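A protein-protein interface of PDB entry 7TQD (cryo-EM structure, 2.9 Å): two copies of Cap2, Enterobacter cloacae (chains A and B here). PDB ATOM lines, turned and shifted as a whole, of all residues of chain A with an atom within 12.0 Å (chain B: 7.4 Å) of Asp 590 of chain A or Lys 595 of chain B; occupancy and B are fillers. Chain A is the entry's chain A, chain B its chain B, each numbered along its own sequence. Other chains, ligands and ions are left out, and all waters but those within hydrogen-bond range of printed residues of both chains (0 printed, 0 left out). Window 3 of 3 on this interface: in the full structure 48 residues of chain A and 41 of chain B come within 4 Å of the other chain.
OE1 of Glu 583 of chain B lies within salt-bridge range of NH2 of Arg 573 of chain B (3.6 Å).
OD1 of Asp 590 of chain A lies within hydrogen-bond range of OG1 of Thr 592 of chain A.
The side-chain carboxylate (OE2) of Glu 583 of chain B is in salt-bridge range of the side-chain amino group (NZ) of Lys 595 of chain B (2.8 Å).
Val 593 of chain A touches its own counterpart, Val 593 of chain B.
Positions printed for both chains: 586, 593, 594 and 595.
Of chain B, only Arg 573, Phe 585 and Lys 595 come within 4 Å of Asp 590 of chain A.
Printed residues of chain A within 4 Å of Lys 595 of chain B: Asp 590 (3.6 Å) and Thr 592 (3.7 Å).
Glu 583 of chain B touches none of the printed residues of chain A.
Of the printed residues of chain A, Phe 585 of chain B touches Asp 590.
No residue of chain A comes within 4 Å of Glu 594 of chain B.
No residue of chain A comes within 4 Å of Glu 596 of chain B.
Printed residues of chain B within 4 Å of Pro 589 of chain A: Arg 573.
Of the printed residues of chain B, Thr 592 of chain A touches Val 593 (3.4 Å) and Lys 595 (3.7 Å).
Of the printed residues of chain B, Val 593 of chain A touches Val 593.
Of the printed residues of chain A, Arg 573 of chain B touches Pro 589 and Asp 590.
The nearest residue of chain A that does not touch Lys 595 of chain B is Gly 591 of chain A (5.5 Å).
N of Val 593 of chain A sits at hydrogen-bond distance from O of Val 593 of chain B (3.2 Å).
Arg 573 of chain B touches Pro 589 of chain A (NH1 to O, 3.9 Å).
Asp 590 of chain A touches Arg 573 of chain B (O to NH2, 3.7 Å).
Asp 590 of chain A touches Phe 585 of chain B.
CD of Lys 595 of chain B touches O of Asp 590 of chain A (3.6 Å).
Thr 592 of chain A touches Val 593 of chain B (CB to O, 3.4 Å).
CB of Lys 595 of chain B touches CG2 of Thr 592 of chain A (3.7 Å).
Hydrophobic or aromatic side chains of chain B that line the printed part of chain A: Phe 585.
Of the 15 printed residues of chain A, 4 touch a printed residue of chain B.
Printed residues of chain A that touch a printed residue of chain B: Pro 589, Asp 590, Thr 592 and Val 593.
Among the printed residues, 7 pairs touch across the chains.
Among the printed residues, no Asp or Glu carboxylate lies within 4 Å of a Lys or Arg side-chain nitrogen of the other chain.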
ATOM      1  N   GLU A 507       7.792   4.841  23.348  1.00  0.00           N
ATOM      2  CA  GLU A 507       7.076   4.298  22.203  1.00  0.00           C
ATOM      3  C   GLU A 507       7.860   4.392  20.903  1.00  0.00           C
ATOM      4  O   GLU A 507       7.509   3.711  19.935  1.00  0.00           O
ATOM      5  CB  GLU A 507       5.734   5.018  22.041  1.00  0.00           C
ATOM      6  CG  GLU A 507       4.746   4.300  21.150  1.00  0.00           C
ATOM      7  CD  GLU A 507       3.352   4.865  21.268  1.00  0.00           C
ATOM      8  OE1 GLU A 507       3.047   5.478  22.312  1.00  0.00           O
ATOM      9  OE2 GLU A 507       2.562   4.701  20.316  1.00  0.00           O
ATOM     10  N   ASP A 558      12.454  -3.448  29.638  1.00  0.00           N
ATOM     11  CA  ASP A 558      12.480  -4.155  28.361  1.00  0.00           C
ATOM     12  C   ASP A 558      12.447  -3.189  27.182  1.00  0.00           C
ATOM     13  O   ASP A 558      13.106  -3.425  26.162  1.00  0.00           O
ATOM     14  CB  ASP A 558      11.324  -5.151  28.291  1.00  0.00           C
ATOM     15  CG  ASP A 558      10.036  -4.582  28.831  1.00  0.00           C
ATOM     16  OD1 ASP A 558      10.041  -3.404  29.230  1.00  0.00           O
ATOM     17  OD2 ASP A 558       9.025  -5.307  28.864  1.00  0.00           O
ATOM     18  N   ASP A 559      11.687  -2.096  27.296  1.00  0.00           N
ATOM     19  CA  ASP A 559      11.685  -1.093  26.234  1.00  0.00           C
ATOM     20  C   ASP A 559      13.067  -0.487  26.048  1.00  0.00           C
ATOM     21  O   ASP A 559      13.537  -0.314  24.915  1.00  0.00           O
ATOM     22  CB  ASP A 559      10.667   0.006  26.536  1.00  0.00           C
ATOM     23  CG  ASP A 559       9.321  -0.543  26.951  1.00  0.00           C
ATOM     24  OD1 ASP A 559       8.908  -1.588  26.409  1.00  0.00           O
ATOM     25  OD2 ASP A 559       8.668   0.077  27.815  1.00  0.00           O
ATOM     26  N   LEU A 562      15.326  -3.006  24.305  1.00  0.00           N
ATOM     27  CA  LEU A 562      15.011  -3.055  22.880  1.00  0.00           C
ATOM     28  C   LEU A 562      15.646  -1.883  22.145  1.00  0.00           C
ATOM     29  O   LEU A 562      16.319  -2.059  21.117  1.00  0.00           O
ATOM     30  CB  LEU A 562      13.492  -3.049  22.693  1.00  0.00           C
ATOM     31  CG  LEU A 562      12.879  -3.168  21.299  1.00  0.00           C
ATOM     32  CD1 LEU A 562      12.848  -4.610  20.846  1.00  0.00           C
ATOM     33  CD2 LEU A 562      11.480  -2.583  21.284  1.00  0.00           C
ATOM     34  N   TRP A 563      15.452  -0.671  22.671  1.00  0.00           N
ATOM     35  CA  TRP A 563      15.988   0.503  21.998  1.00  0.00           C
ATOM     36  C   TRP A 563      17.508   0.553  22.066  1.00  0.00           C
ATOM     37  O   TRP A 563      18.142   1.083  21.152  1.00  0.00           O
ATOM     38  CB  TRP A 563      15.370   1.770  22.578  1.00  0.00           C
ATOM     39  CG  TRP A 563      13.892   1.875  22.338  1.00  0.00           C
ATOM     40  CD1 TRP A 563      12.948   2.248  23.242  1.00  0.00           C
ATOM     41  CD2 TRP A 563      13.188   1.606  21.114  1.00  0.00           C
ATOM     42  NE1 TRP A 563      11.703   2.228  22.666  1.00  0.00           N
ATOM     43  CE2 TRP A 563      11.825   1.839  21.359  1.00  0.00           C
ATOM     44  CE3 TRP A 563      13.579   1.194  19.835  1.00  0.00           C
ATOM     45  CZ2 TRP A 563      10.851   1.671  20.378  1.00  0.00           C
ATOM     46  CZ3 TRP A 563      12.614   1.027  18.866  1.00  0.00           C
ATOM     47  CH2 TRP A 563      11.265   1.264  19.142  1.00  0.00           C
ATOM     48  N   LYS A 586       9.471   2.794  15.567  1.00  0.00           N
ATOM     49  CA  LYS A 586       8.237   2.703  16.333  1.00  0.00           C
ATOM     50  C   LYS A 586       7.988   1.251  16.705  1.00  0.00           C
ATOM     51  O   LYS A 586       8.196   0.358  15.880  1.00  0.00           O
ATOM     52  CB  LYS A 586       7.054   3.256  15.531  1.00  0.00           C
ATOM     53  CG  LYS A 586       5.730   3.210  16.263  1.00  0.00           C
ATOM     54  CD  LYS A 586       4.588   3.654  15.366  1.00  0.00           C
ATOM     55  CE  LYS A 586       3.271   3.684  16.126  1.00  0.00           C
ATOM     56  NZ  LYS A 586       2.134   4.104  15.262  1.00  0.00           N
ATOM     57  N   GLN A 587       7.544   1.017  17.936  1.00  0.00           N
ATOM     58  CA  GLN A 587       7.178  -0.320  18.375  1.00  0.00           C
ATOM     59  C   GLN A 587       5.663  -0.471  18.388  1.00  0.00           C
ATOM     60  O   GLN A 587       4.927   0.463  18.717  1.00  0.00           O
ATOM     61  CB  GLN A 587       7.755  -0.625  19.759  1.00  0.00           C
ATOM     62  CG  GLN A 587       7.143   0.169  20.900  1.00  0.00           C
ATOM     63  CD  GLN A 587       7.603  -0.317  22.261  1.00  0.00           C
ATOM     64  OE1 GLN A 587       8.562  -1.078  22.370  1.00  0.00           O
ATOM     65  NE2 GLN A 587       6.916   0.122  23.307  1.00  0.00           N
ATOM     66  N   MET A 588       5.201  -1.661  18.013  1.00  0.00           N
ATOM     67  CA  MET A 588       3.782  -1.931  17.864  1.00  0.00           C
ATOM     68  C   MET A 588       3.292  -2.879  18.956  1.00  0.00           C
ATOM     69  O   MET A 588       4.088  -3.621  19.540  1.00  0.00           O
ATOM     70  CB  MET A 588       3.490  -2.540  16.488  1.00  0.00           C
ATOM     71  CG  MET A 588       4.027  -1.721  15.331  1.00  0.00           C
ATOM     72  SD  MET A 588       3.321  -0.070  15.260  1.00  0.00           S
ATOM     73  CE  MET A 588       1.612  -0.457  14.902  1.00  0.00           C
ATOM     74  N   PRO A 589       1.993  -2.863  19.270  1.00  0.00           N
ATOM     75  CA  PRO A 589       1.493  -3.724  20.356  1.00  0.00           C
ATOM     76  C   PRO A 589       1.733  -5.207  20.133  1.00  0.00           C
ATOM     77  O   PRO A 589       1.909  -5.947  21.109  1.00  0.00           O
ATOM     78  CB  PRO A 589      -0.005  -3.397  20.395  1.00  0.00           C
ATOM     79  CG  PRO A 589      -0.103  -2.030  19.822  1.00  0.00           C
ATOM     80  CD  PRO A 589       0.947  -1.961  18.760  1.00  0.00           C
ATOM     81  N   ASP A 590       1.747  -5.672  18.882  1.00  0.00           N
ATOM     82  CA  ASP A 590       1.951  -7.091  18.618  1.00  0.00           C
ATOM     83  C   ASP A 590       3.405  -7.517  18.755  1.00  0.00           C
ATOM     84  O   ASP A 590       3.694  -8.711  18.633  1.00  0.00           O
ATOM     85  CB  ASP A 590       1.430  -7.447  17.225  1.00  0.00           C
ATOM     86  CG  ASP A 590       2.028  -6.578  16.136  1.00  0.00           C
ATOM     87  OD1 ASP A 590       2.883  -5.728  16.451  1.00  0.00           O
ATOM     88  OD2 ASP A 590       1.640  -6.745  14.962  1.00  0.00           O
ATOM     89  N   GLY A 591       4.319  -6.584  18.998  1.00  0.00           N
ATOM     90  CA  GLY A 591       5.718  -6.905  19.180  1.00  0.00           C
ATOM     91  C   GLY A 591       6.619  -6.600  18.003  1.00  0.00           C
ATOM     92  O   GLY A 591       7.793  -6.980  18.036  1.00  0.00           O
ATOM     93  N   THR A 592       6.116  -5.927  16.973  1.00  0.00           N
ATOM     94  CA  THR A 592       6.890  -5.612  15.783  1.00  0.00           C
ATOM     95  C   THR A 592       7.488  -4.213  15.877  1.00  0.00           C
ATOM     96  O   THR A 592       7.023  -3.358  16.634  1.00  0.00           O
ATOM     97  CB  THR A 592       6.022  -5.706  14.527  1.00  0.00           C
ATOM     98  OG1 THR A 592       4.969  -4.740  14.602  1.00  0.00           O
ATOM     99  CG2 THR A 592       5.422  -7.090  14.392  1.00  0.00           C
ATOM    100  N   VAL A 593       8.522  -3.989  15.074  1.00  0.00           N
ATOM    101  CA  VAL A 593       9.224  -2.716  15.006  1.00  0.00           C
ATOM    102  C   VAL A 593       9.138  -2.202  13.576  1.00  0.00           C
ATOM    103  O   VAL A 593       9.472  -2.926  12.633  1.00  0.00           O
ATOM    104  CB  VAL A 593      10.691  -2.859  15.450  1.00  0.00           C
ATOM    105  CG1 VAL A 593      11.425  -1.542  15.303  1.00  0.00           C
ATOM    106  CG2 VAL A 593      10.762  -3.356  16.882  1.00  0.00           C
ATOM    107  N   GLU A 594       8.686  -0.963  13.419  1.00  0.00           N
ATOM    108  CA  GLU A 594       8.598  -0.313  12.120  1.00  0.00           C
ATOM    109  C   GLU A 594       9.543   0.880  12.074  1.00  0.00           C
ATOM    110  O   GLU A 594       9.874   1.469  13.105  1.00  0.00           O
ATOM    111  CB  GLU A 594       7.165   0.138  11.823  1.00  0.00           C
ATOM    112  CG  GLU A 594       6.147  -0.986  11.849  1.00  0.00           C
ATOM    113  CD  GLU A 594       4.724  -0.494  11.665  1.00  0.00           C
ATOM    114  OE1 GLU A 594       4.528   0.731  11.524  1.00  0.00           O
ATOM    115  OE2 GLU A 594       3.801  -1.334  11.655  1.00  0.00           O
ATOM    116  N   LYS A 595       9.980   1.229  10.868  1.00  0.00           N
ATOM    117  CA  LYS A 595      10.969   2.278  10.671  1.00  0.00           C
ATOM    118  C   LYS A 595      10.497   3.262   9.613  1.00  0.00           C
ATOM    119  O   LYS A 595       9.982   2.862   8.566  1.00  0.00           O
ATOM    120  CB  LYS A 595      12.316   1.681  10.263  1.00  0.00           C
ATOM    121  CG  LYS A 595      13.227   2.632   9.517  1.00  0.00           C
ATOM    122  CD  LYS A 595      14.464   1.905   9.040  1.00  0.00           C
ATOM    123  CE  LYS A 595      15.125   2.626   7.886  1.00  0.00           C
ATOM    124  NZ  LYS A 595      16.359   1.915   7.457  1.00  0.00           N
ATOM    125  N   VAL B 566      11.939  -9.001  23.548  1.00  0.00           N
ATOM    126  CA  VAL B 566      10.724  -9.459  22.880  1.00  0.00           C
ATOM    127  C   VAL B 566      10.090 -10.610  23.653  1.00  0.00           C
ATOM    128  O   VAL B 566       8.865 -10.672  23.807  1.00  0.00           O
ATOM    129  CB  VAL B 566      11.026  -9.849  21.420  1.00  0.00           C
ATOM    130  CG1 VAL B 566       9.782 -10.398  20.758  1.00  0.00           C
ATOM    131  CG2 VAL B 566      11.542  -8.650  20.652  1.00  0.00           C
ATOM    132  N   PHE B 570       6.417 -10.868  25.375  1.00  0.00           N
ATOM    133  CA  PHE B 570       5.549 -11.994  25.042  1.00  0.00           C
ATOM    134  C   PHE B 570       5.063 -12.710  26.296  1.00  0.00           C
ATOM    135  O   PHE B 570       3.892 -13.090  26.387  1.00  0.00           O
ATOM    136  CB  PHE B 570       6.294 -12.955  24.116  1.00  0.00           C
ATOM    137  CG  PHE B 570       5.545 -14.217  23.806  1.00  0.00           C
ATOM    138  CD1 PHE B 570       4.493 -14.212  22.906  1.00  0.00           C
ATOM    139  CD2 PHE B 570       5.903 -15.414  24.400  1.00  0.00           C
ATOM    140  CE1 PHE B 570       3.807 -15.375  22.613  1.00  0.00           C
ATOM    141  CE2 PHE B 570       5.222 -16.576  24.115  1.00  0.00           C
ATOM    142  CZ  PHE B 570       4.173 -16.558  23.220  1.00  0.00           C
ATOM    143  N   ARG B 573       2.356 -10.596  27.906  1.00  0.00           N
ATOM    144  CA  ARG B 573       1.092 -10.684  27.180  1.00  0.00           C
ATOM    145  C   ARG B 573       0.404 -12.023  27.410  1.00  0.00           C
ATOM    146  O   ARG B 573      -0.821 -12.082  27.566  1.00  0.00           O
ATOM    147  CB  ARG B 573       1.317 -10.457  25.688  1.00  0.00           C
ATOM    148  CG  ARG B 573       1.641  -9.028  25.317  1.00  0.00           C
ATOM    149  CD  ARG B 573       1.379  -8.784  23.842  1.00  0.00           C
ATOM    150  NE  ARG B 573       2.065  -9.758  23.004  1.00  0.00           N
ATOM    151  CZ  ARG B 573       3.324  -9.647  22.601  1.00  0.00           C
ATOM    152  NH1 ARG B 573       4.072  -8.614  22.948  1.00  0.00           N
ATOM    153  NH2 ARG B 573       3.843 -10.598  21.831  1.00  0.00           N
ATOM    154  N   ILE B 581      -1.157 -20.174  22.149  1.00  0.00           N
ATOM    155  CA  ILE B 581      -0.645 -19.135  21.264  1.00  0.00           C
ATOM    156  C   ILE B 581       0.701 -19.574  20.707  1.00  0.00           C
ATOM    157  O   ILE B 581       1.531 -20.134  21.433  1.00  0.00           O
ATOM    158  CB  ILE B 581      -0.506 -17.779  21.992  1.00  0.00           C
ATOM    159  CG1 ILE B 581      -1.745 -17.490  22.841  1.00  0.00           C
ATOM    160  CG2 ILE B 581      -0.280 -16.659  20.995  1.00  0.00           C
ATOM    161  CD1 ILE B 581      -1.577 -16.334  23.798  1.00  0.00           C
ATOM    162  N   TYR B 582       0.916 -19.322  19.416  1.00  0.00           N
ATOM    163  CA  TYR B 582       2.210 -19.544  18.786  1.00  0.00           C
ATOM    164  C   TYR B 582       2.514 -18.385  17.848  1.00  0.00           C
ATOM    165  O   TYR B 582       1.652 -17.966  17.073  1.00  0.00           O
ATOM    166  CB  TYR B 582       2.248 -20.864  18.014  1.00  0.00           C
ATOM    167  CG  TYR B 582       3.566 -21.111  17.319  1.00  0.00           C
ATOM    168  CD1 TYR B 582       4.690 -21.501  18.037  1.00  0.00           C
ATOM    169  CD2 TYR B 582       3.692 -20.947  15.948  1.00  0.00           C
ATOM    170  CE1 TYR B 582       5.897 -21.725  17.409  1.00  0.00           C
ATOM    171  CE2 TYR B 582       4.897 -21.168  15.311  1.00  0.00           C
ATOM    172  CZ  TYR B 582       5.996 -21.556  16.047  1.00  0.00           C
ATOM    173  OH  TYR B 582       7.197 -21.776  15.416  1.00  0.00           O
ATOM    174  N   GLU B 583       3.743 -17.873  17.924  1.00  0.00           N
ATOM    175  CA  GLU B 583       4.167 -16.737  17.119  1.00  0.00           C
ATOM    176  C   GLU B 583       5.604 -16.943  16.665  1.00  0.00           C
ATOM    177  O   GLU B 583       6.403 -17.582  17.354  1.00  0.00           O
ATOM    178  CB  GLU B 583       4.054 -15.419  17.900  1.00  0.00           C
ATOM    179  CG  GLU B 583       2.630 -14.924  18.094  1.00  0.00           C
ATOM    180  CD  GLU B 583       2.531 -13.814  19.125  1.00  0.00           C
ATOM    181  OE1 GLU B 583       3.560 -13.477  19.748  1.00  0.00           O
ATOM    182  OE2 GLU B 583       1.420 -13.278  19.313  1.00  0.00           O
ATOM    183  N   TYR B 584       5.929 -16.392  15.497  1.00  0.00           N
ATOM    184  CA  TYR B 584       7.275 -16.451  14.944  1.00  0.00           C
ATOM    185  C   TYR B 584       7.717 -15.052  14.540  1.00  0.00           C
ATOM    186  O   TYR B 584       7.048 -14.396  13.736  1.00  0.00           O
ATOM    187  CB  TYR B 584       7.335 -17.396  13.741  1.00  0.00           C
ATOM    188  CG  TYR B 584       8.702 -17.488  13.108  1.00  0.00           C
ATOM    189  CD1 TYR B 584       9.724 -18.193  13.721  1.00  0.00           C
ATOM    190  CD2 TYR B 584       8.971 -16.869  11.899  1.00  0.00           C
ATOM    191  CE1 TYR B 584      10.972 -18.280  13.149  1.00  0.00           C
ATOM    192  CE2 TYR B 584      10.219 -16.951  11.319  1.00  0.00           C
ATOM    193  CZ  TYR B 584      11.216 -17.658  11.950  1.00  0.00           C
ATOM    194  OH  TYR B 584      12.461 -17.743  11.378  1.00  0.00           O
ATOM    195  N   PHE B 585       8.848 -14.606  15.087  1.00  0.00           N
ATOM    196  CA  PHE B 585       9.379 -13.272  14.848  1.00  0.00           C
ATOM    197  C   PHE B 585      10.665 -13.362  14.041  1.00  0.00           C
ATOM    198  O   PHE B 585      11.428 -14.321  14.179  1.00  0.00           O
ATOM    199  CB  PHE B 585       9.655 -12.533  16.160  1.00  0.00           C
ATOM    200  CG  PHE B 585       8.436 -12.312  17.005  1.00  0.00           C
ATOM    201  CD1 PHE B 585       7.603 -11.235  16.772  1.00  0.00           C
ATOM    202  CD2 PHE B 585       8.127 -13.178  18.037  1.00  0.00           C
ATOM    203  CE1 PHE B 585       6.486 -11.028  17.548  1.00  0.00           C
ATOM    204  CE2 PHE B 585       7.010 -12.976  18.814  1.00  0.00           C
ATOM    205  CZ  PHE B 585       6.190 -11.899  18.570  1.00  0.00           C
ATOM    206  N   LYS B 586      10.906 -12.353  13.206  1.00  0.00           N
ATOM    207  CA  LYS B 586      12.051 -12.337  12.307  1.00  0.00           C
ATOM    208  C   LYS B 586      12.624 -10.930  12.237  1.00  0.00           C
ATOM    209  O   LYS B 586      11.868  -9.961  12.124  1.00  0.00           O
ATOM    210  CB  LYS B 586      11.644 -12.812  10.909  1.00  0.00           C
ATOM    211  CG  LYS B 586      12.742 -12.747   9.871  1.00  0.00           C
ATOM    212  CD  LYS B 586      12.181 -12.975   8.478  1.00  0.00           C
ATOM    213  CE  LYS B 586      13.270 -12.895   7.424  1.00  0.00           C
ATOM    214  NZ  LYS B 586      12.724 -13.036   6.047  1.00  0.00           N
ATOM    215  N   VAL B 593      11.609  -5.610  12.852  1.00  0.00           N
ATOM    216  CA  VAL B 593      11.242  -6.951  13.289  1.00  0.00           C
ATOM    217  C   VAL B 593       9.827  -7.230  12.805  1.00  0.00           C
ATOM    218  O   VAL B 593       8.938  -6.386  12.959  1.00  0.00           O
ATOM    219  CB  VAL B 593      11.341  -7.096  14.819  1.00  0.00           C
ATOM    220  CG1 VAL B 593      10.720  -8.401  15.279  1.00  0.00           C
ATOM    221  CG2 VAL B 593      12.791  -7.008  15.271  1.00  0.00           C
ATOM    222  N   GLU B 594       9.620  -8.406  12.217  1.00  0.00           N
ATOM    223  CA  GLU B 594       8.324  -8.793  11.677  1.00  0.00           C
ATOM    224  C   GLU B 594       7.821 -10.061  12.357  1.00  0.00           C
ATOM    225  O   GLU B 594       8.607 -10.911  12.784  1.00  0.00           O
ATOM    226  CB  GLU B 594       8.409  -9.009  10.165  1.00  0.00           C
ATOM    227  CG  GLU B 594       8.840  -7.775   9.391  1.00  0.00           C
ATOM    228  CD  GLU B 594       9.066  -8.058   7.921  1.00  0.00           C
ATOM    229  OE1 GLU B 594       8.895  -9.223   7.508  1.00  0.00           O
ATOM    230  OE2 GLU B 594       9.418  -7.117   7.179  1.00  0.00           O
ATOM    231  N   LYS B 595       6.496 -10.179  12.451  1.00  0.00           N
ATOM    232  CA  LYS B 595       5.844 -11.267  13.169  1.00  0.00           C
ATOM    233  C   LYS B 595       4.932 -12.043  12.233  1.00  0.00           C
ATOM    234  O   LYS B 595       4.251 -11.455  11.389  1.00  0.00           O
ATOM    235  CB  LYS B 595       5.027 -10.738  14.358  1.00  0.00           C
ATOM    236  CG  LYS B 595       3.960 -11.692  14.880  1.00  0.00           C
ATOM    237  CD  LYS B 595       3.180 -11.062  16.018  1.00  0.00           C
ATOM    238  CE  LYS B 595       1.872 -11.785  16.280  1.00  0.00           C
ATOM    239  NZ  LYS B 595       1.159 -11.197  17.448  1.00  0.00           N
ATOM    240  N   GLU B 596       4.918 -13.363  12.391  1.00  0.00           N
ATOM    241  CA  GLU B 596       3.998 -14.211  11.639  1.00  0.00           C
ATOM    242  C   GLU B 596       3.152 -15.075  12.573  1.00  0.00           C
ATOM    243  O   GLU B 596       3.682 -15.792  13.422  1.00  0.00           O
ATOM    244  CB  GLU B 596       4.761 -15.097  10.660  1.00  0.00           C
ATOM    245  CG  GLU B 596       5.756 -14.349   9.798  1.00  0.00           C
ATOM    246  CD  GLU B 596       6.816 -15.263   9.227  1.00  0.00           C
ATOM    247  OE1 GLU B 596       6.707 -16.491   9.427  1.00  0.00           O
ATOM    248  OE2 GLU B 596       7.757 -14.757   8.582  1.00  0.00           O
